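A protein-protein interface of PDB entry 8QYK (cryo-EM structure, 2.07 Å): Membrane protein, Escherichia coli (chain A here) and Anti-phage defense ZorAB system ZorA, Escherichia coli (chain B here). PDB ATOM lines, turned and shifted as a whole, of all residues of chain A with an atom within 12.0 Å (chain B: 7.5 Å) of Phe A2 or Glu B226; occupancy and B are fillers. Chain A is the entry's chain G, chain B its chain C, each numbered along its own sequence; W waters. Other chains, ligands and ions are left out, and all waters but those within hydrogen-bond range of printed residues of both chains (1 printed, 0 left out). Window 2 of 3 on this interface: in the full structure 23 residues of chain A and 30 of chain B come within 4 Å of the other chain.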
ATOM      1  N   MET A   1      13.618 -20.577  17.387  1.00  0.00           N
ATOM      2  CA  MET A   1      14.615 -19.645  17.895  1.00  0.00           C
ATOM      3  C   MET A   1      14.005 -18.694  18.919  1.00  0.00           C
ATOM      4  O   MET A   1      14.461 -18.620  20.059  1.00  0.00           O
ATOM      5  CB  MET A   1      15.237 -18.854  16.746  1.00  0.00           C
ATOM      6  CG  MET A   1      16.397 -17.964  17.155  1.00  0.00           C
ATOM      7  SD  MET A   1      17.835 -18.884  17.728  1.00  0.00           S
ATOM      8  CE  MET A   1      18.639 -17.650  18.743  1.00  0.00           C
ATOM      9  N   PHE A   2      12.975 -17.963  18.504  1.00  0.00           N
ATOM     10  CA  PHE A   2      12.242 -17.056  19.381  1.00  0.00           C
ATOM     11  C   PHE A   2      10.787 -17.487  19.471  1.00  0.00           C
ATOM     12  O   PHE A   2       9.862 -16.672  19.438  1.00  0.00           O
ATOM     13  CB  PHE A   2      12.341 -15.613  18.897  1.00  0.00           C
ATOM     14  CG  PHE A   2      13.685 -14.984  19.125  1.00  0.00           C
ATOM     15  CD1 PHE A   2      14.053 -14.523  20.375  1.00  0.00           C
ATOM     16  CD2 PHE A   2      14.575 -14.840  18.077  1.00  0.00           C
ATOM     17  CE1 PHE A   2      15.290 -13.942  20.569  1.00  0.00           C
ATOM     18  CE2 PHE A   2      15.806 -14.259  18.268  1.00  0.00           C
ATOM     19  CZ  PHE A   2      16.164 -13.808  19.516  1.00  0.00           C
ATOM     20  N   GLY A   3      10.569 -18.795  19.570  1.00  0.00           N
ATOM     21  CA  GLY A   3       9.223 -19.308  19.683  1.00  0.00           C
ATOM     22  C   GLY A   3       8.578 -18.935  21.003  1.00  0.00           C
ATOM     23  O   GLY A   3       9.239 -18.632  21.996  1.00  0.00           O
ATOM     24  N   ASN A   4       7.251 -18.955  21.005  1.00  0.00           N
ATOM     25  CA  ASN A   4       6.472 -18.560  22.170  1.00  0.00           C
ATOM     26  C   ASN A   4       6.345 -19.747  23.117  1.00  0.00           C
ATOM     27  O   ASN A   4       5.742 -20.768  22.765  1.00  0.00           O
ATOM     28  CB  ASN A   4       5.097 -18.047  21.743  1.00  0.00           C
ATOM     29  CG  ASN A   4       4.168 -17.813  22.917  1.00  0.00           C
ATOM     30  OD1 ASN A   4       4.597 -17.389  23.991  1.00  0.00           O
ATOM     31  ND2 ASN A   4       2.883 -18.074  22.712  1.00  0.00           N
ATOM     32  N   ALA A   5       6.920 -19.614  24.314  1.00  0.00           N
ATOM     33  CA  ALA A   5       6.829 -20.678  25.307  1.00  0.00           C
ATOM     34  C   ALA A   5       5.446 -20.764  25.936  1.00  0.00           C
ATOM     35  O   ALA A   5       5.140 -21.760  26.596  1.00  0.00           O
ATOM     36  CB  ALA A   5       7.880 -20.474  26.397  1.00  0.00           C
ATOM     37  N   PHE A   6       4.680 -19.706  25.854  1.00  0.00           N
ATOM     38  CA  PHE A   6       3.384 -19.658  26.572  1.00  0.00           C
ATOM     39  C   PHE A   6       2.262 -20.096  25.627  1.00  0.00           C
ATOM     40  O   PHE A   6       1.087 -20.007  26.014  1.00  0.00           O
ATOM     41  CB  PHE A   6       3.246 -18.297  27.265  1.00  0.00           C
ATOM     42  CG  PHE A   6       4.193 -17.966  28.384  1.00  0.00           C
ATOM     43  CD1 PHE A   6       5.496 -17.575  28.127  1.00  0.00           C
ATOM     44  CD2 PHE A   6       3.770 -18.015  29.697  1.00  0.00           C
ATOM     45  CE1 PHE A   6       6.366 -17.279  29.159  1.00  0.00           C
ATOM     46  CE2 PHE A   6       4.644 -17.715  30.723  1.00  0.00           C
ATOM     47  CZ  PHE A   6       5.938 -17.353  30.456  1.00  0.00           C
ATOM     48  N   GLY A   7       2.593 -20.559  24.434  1.00  0.00           N
ATOM     49  CA  GLY A   7       1.568 -21.116  23.546  1.00  0.00           C
ATOM     50  C   GLY A   7       0.727 -22.064  24.377  1.00  0.00           C
ATOM     51  O   GLY A   7       1.320 -22.956  25.062  1.00  0.00           O
ATOM     52  N   THR B 110       5.560 -10.443  22.003  1.00  0.00           N
ATOM     53  CA  THR B 110       6.378 -11.643  21.941  1.00  0.00           C
ATOM     54  C   THR B 110       5.542 -12.912  21.900  1.00  0.00           C
ATOM     55  O   THR B 110       6.103 -14.007  21.818  1.00  0.00           O
ATOM     56  CB  THR B 110       7.336 -11.696  23.134  1.00  0.00           C
ATOM     57  OG1 THR B 110       6.582 -11.785  24.348  1.00  0.00           O
ATOM     58  CG2 THR B 110       8.217 -10.458  23.168  1.00  0.00           C
ATOM     59  N   ALA B 111       4.219 -12.788  21.955  1.00  0.00           N
ATOM     60  CA  ALA B 111       3.326 -13.936  21.959  1.00  0.00           C
ATOM     61  C   ALA B 111       1.999 -13.513  21.359  1.00  0.00           C
ATOM     62  O   ALA B 111       1.631 -12.338  21.452  1.00  0.00           O
ATOM     63  CB  ALA B 111       3.118 -14.470  23.381  1.00  0.00           C
ATOM     64  N   SER B 222       5.433  -8.078  16.353  1.00  0.00           N
ATOM     65  CA  SER B 222       6.316  -9.126  16.843  1.00  0.00           C
ATOM     66  C   SER B 222       7.705  -8.973  16.230  1.00  0.00           C
ATOM     67  O   SER B 222       8.020  -7.976  15.576  1.00  0.00           O
ATOM     68  CB  SER B 222       5.732 -10.508  16.535  1.00  0.00           C
ATOM     69  OG  SER B 222       4.540 -10.733  17.263  1.00  0.00           O
ATOM     70  N   GLY B 223       8.544  -9.979  16.458  1.00  0.00           N
ATOM     71  CA  GLY B 223       9.851 -10.031  15.838  1.00  0.00           C
ATOM     72  C   GLY B 223      10.897  -9.099  16.403  1.00  0.00           C
ATOM     73  O   GLY B 223      11.850  -8.764  15.695  1.00  0.00           O
ATOM     74  N   VAL B 224      10.758  -8.665  17.656  1.00  0.00           N
ATOM     75  CA  VAL B 224      11.771  -7.786  18.229  1.00  0.00           C
ATOM     76  C   VAL B 224      13.068  -8.544  18.506  1.00  0.00           C
ATOM     77  O   VAL B 224      14.154  -7.962  18.439  1.00  0.00           O
ATOM     78  CB  VAL B 224      11.242  -7.088  19.499  1.00  0.00           C
ATOM     79  CG1 VAL B 224      11.094  -8.074  20.650  1.00  0.00           C
ATOM     80  CG2 VAL B 224      12.164  -5.947  19.890  1.00  0.00           C
ATOM     81  N   GLY B 225      12.986  -9.836  18.830  1.00  0.00           N
ATOM     82  CA  GLY B 225      14.181 -10.573  19.215  1.00  0.00           C
ATOM     83  C   GLY B 225      15.182 -10.712  18.084  1.00  0.00           C
ATOM     84  O   GLY B 225      16.392 -10.556  18.287  1.00  0.00           O
ATOM     85  N   GLU B 226      14.695 -11.008  16.879  1.00  0.00           N
ATOM     86  CA  GLU B 226      15.575 -11.061  15.719  1.00  0.00           C
ATOM     87  C   GLU B 226      16.164  -9.690  15.419  1.00  0.00           C
ATOM     88  O   GLU B 226      17.320  -9.584  14.994  1.00  0.00           O
ATOM     89  CB  GLU B 226      14.815 -11.607  14.511  1.00  0.00           C
ATOM     90  CG  GLU B 226      14.582 -13.107  14.557  1.00  0.00           C
ATOM     91  CD  GLU B 226      13.314 -13.487  15.304  1.00  0.00           C
ATOM     92  OE1 GLU B 226      12.568 -12.580  15.731  1.00  0.00           O
ATOM     93  OE2 GLU B 226      13.063 -14.699  15.461  1.00  0.00           O
ATOM     94  N   GLU B 227      15.391  -8.627  15.643  1.00  0.00           N
ATOM     95  CA  GLU B 227      15.918  -7.278  15.462  1.00  0.00           C
ATOM     96  C   GLU B 227      17.043  -6.986  16.445  1.00  0.00           C
ATOM     97  O   GLU B 227      18.060  -6.392  16.074  1.00  0.00           O
ATOM     98  CB  GLU B 227      14.796  -6.252  15.604  1.00  0.00           C
ATOM     99  CG  GLU B 227      13.733  -6.363  14.532  1.00  0.00           C
ATOM    100  CD  GLU B 227      12.571  -5.419  14.756  1.00  0.00           C
ATOM    101  OE1 GLU B 227      12.623  -4.626  15.717  1.00  0.00           O
ATOM    102  OE2 GLU B 227      11.606  -5.470  13.966  1.00  0.00           O
ATOM    103  N   TYR B 228      16.875  -7.395  17.706  1.00  0.00           N
ATOM    104  CA  TYR B 228      17.928  -7.213  18.700  1.00  0.00           C
ATOM    105  C   TYR B 228      19.179  -7.995  18.325  1.00  0.00           C
ATOM    106  O   TYR B 228      20.301  -7.491  18.457  1.00  0.00           O
ATOM    107  CB  TYR B 228      17.434  -7.640  20.081  1.00  0.00           C
ATOM    108  CG  TYR B 228      16.511  -6.657  20.760  1.00  0.00           C
ATOM    109  CD1 TYR B 228      16.544  -5.306  20.448  1.00  0.00           C
ATOM    110  CD2 TYR B 228      15.604  -7.083  21.719  1.00  0.00           C
ATOM    111  CE1 TYR B 228      15.703  -4.411  21.067  1.00  0.00           C
ATOM    112  CE2 TYR B 228      14.759  -6.194  22.345  1.00  0.00           C
ATOM    113  CZ  TYR B 228      14.813  -4.861  22.015  1.00  0.00           C
ATOM    114  OH  TYR B 228      13.974  -3.970  22.635  1.00  0.00           O
ATOM    115  N   LEU B 229      19.006  -9.236  17.864  1.00  0.00           N
ATOM    116  CA  LEU B 229      20.157 -10.033  17.445  1.00  0.00           C
ATOM    117  C   LEU B 229      20.875  -9.395  16.260  1.00  0.00           C
ATOM    118  O   LEU B 229      22.111  -9.347  16.228  1.00  0.00           O
ATOM    119  CB  LEU B 229      19.715 -11.455  17.103  1.00  0.00           C
ATOM    120  CG  LEU B 229      19.487 -12.416  18.269  1.00  0.00           C
ATOM    121  CD1 LEU B 229      19.380 -13.844  17.764  1.00  0.00           C
ATOM    122  CD2 LEU B 229      20.593 -12.295  19.303  1.00  0.00           C
ATOM    123  N   ALA B 230      20.117  -8.898  15.280  1.00  0.00           N
ATOM    124  CA  ALA B 230      20.720  -8.228  14.134  1.00  0.00           C
ATOM    125  C   ALA B 230      21.465  -6.967  14.559  1.00  0.00           C
ATOM    126  O   ALA B 230      22.560  -6.680  14.055  1.00  0.00           O
ATOM    127  CB  ALA B 230      19.646  -7.902  13.098  1.00  0.00           C
ATOM    128  N   SER B 231      20.884  -6.202  15.488  1.00  0.00           N
ATOM    129  CA  SER B 231      21.565  -5.028  16.022  1.00  0.00           C
ATOM    130  C   SER B 231      22.868  -5.414  16.707  1.00  0.00           C
ATOM    131  O   SER B 231      23.882  -4.730  16.549  1.00  0.00           O
ATOM    132  CB  SER B 231      20.653  -4.284  16.996  1.00  0.00           C
ATOM    133  OG  SER B 231      19.711  -3.487  16.309  1.00  0.00           O
ATOM    134  N   LEU B 232      22.859  -6.511  17.466  1.00  0.00           N
ATOM    135  CA  LEU B 232      24.081  -6.956  18.131  1.00  0.00           C
ATOM    136  C   LEU B 232      25.147  -7.355  17.120  1.00  0.00           C
ATOM    137  O   LEU B 232      26.330  -7.047  17.303  1.00  0.00           O
ATOM    138  CB  LEU B 232      23.783  -8.120  19.075  1.00  0.00           C
ATOM    139  CG  LEU B 232      23.045  -7.808  20.376  1.00  0.00           C
ATOM    140  CD1 LEU B 232      22.805  -9.081  21.160  1.00  0.00           C
ATOM    141  CD2 LEU B 232      23.812  -6.793  21.207  1.00  0.00           C
ATOM    142  N   VAL B 233      24.749  -8.048  16.052  1.00  0.00           N
ATOM    143  CA  VAL B 233      25.709  -8.467  15.031  1.00  0.00           C
ATOM    144  C   VAL B 233      26.334  -7.249  14.359  1.00  0.00           C
ATOM    145  O   VAL B 233      27.564  -7.153  14.200  1.00  0.00           O
ATOM    146  CB  VAL B 233      25.023  -9.388  14.005  1.00  0.00           C
ATOM    147  CG1 VAL B 233      25.911  -9.604  12.794  1.00  0.00           C
ATOM    148  CG2 VAL B 233      24.648 -10.712  14.646  1.00  0.00           C
HETATM  149  O   HOH W   1       5.855 -14.896  25.185  1.00  0.00           O
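Of the 7 printed residues of chain A, 3 touch a printed residue of chain B.
Hydrophobic or aromatic side chains of chain A within 4 Å of the printed part of chain B: Met A1 and Phe A2.
Among the printed residues, 5 pairs touch across the chains.
N of Phe A6 sits at hydrogen-bond distance from OD1 of Asn A4 (3.0 Å).
ND2 of Asn A4 lies close to N of Gly A7 (3.0 Å).
Water W1 lies within hydrogen-bond range of the side-chain amide oxygen (OD1) of Asn A4 and the side-chain hydroxyl (OG1) of Thr B110.
Among the printed residues, pairs that only touch across the chains: Met A1 with Leu B229 (3.999 Å), Phe A2 with Gly B225 (3.5 Å), Phe A2 with Glu B226 (3.0 Å), Phe A2 with Leu B229 (3.6 Å) and Asn A4 with Ala B111 (3.3 Å).
Of chain B, only Gly B225, Glu B226 and Leu B229 come within 4 Å of Phe A2.
Printed residues of chain B within 4 Å of Asn A4: Ala B111 (3.3 Å).
Ala A5 touches none of the printed residues of chain B.
No residue of chain A comes within 4 Å of Val B224.
Gly B225 touches one residue of chain A.
Of chain A, only Phe A2 comes within 4 Å of Glu B226.
No residue of chain A comes within 4 Å of Glu B227.
Of the printed residues of chain A, Leu B229 touches Met A1 and Phe A2.
No residue of chain A comes within 4 Å of Ala B230.
The nearest residue of chain A that does not touch Glu B226 is Met A1 (4.9 Å).
The nearest printed residue of chain B that does not touch Asn A4 is Thr B110 (4.2 Å).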
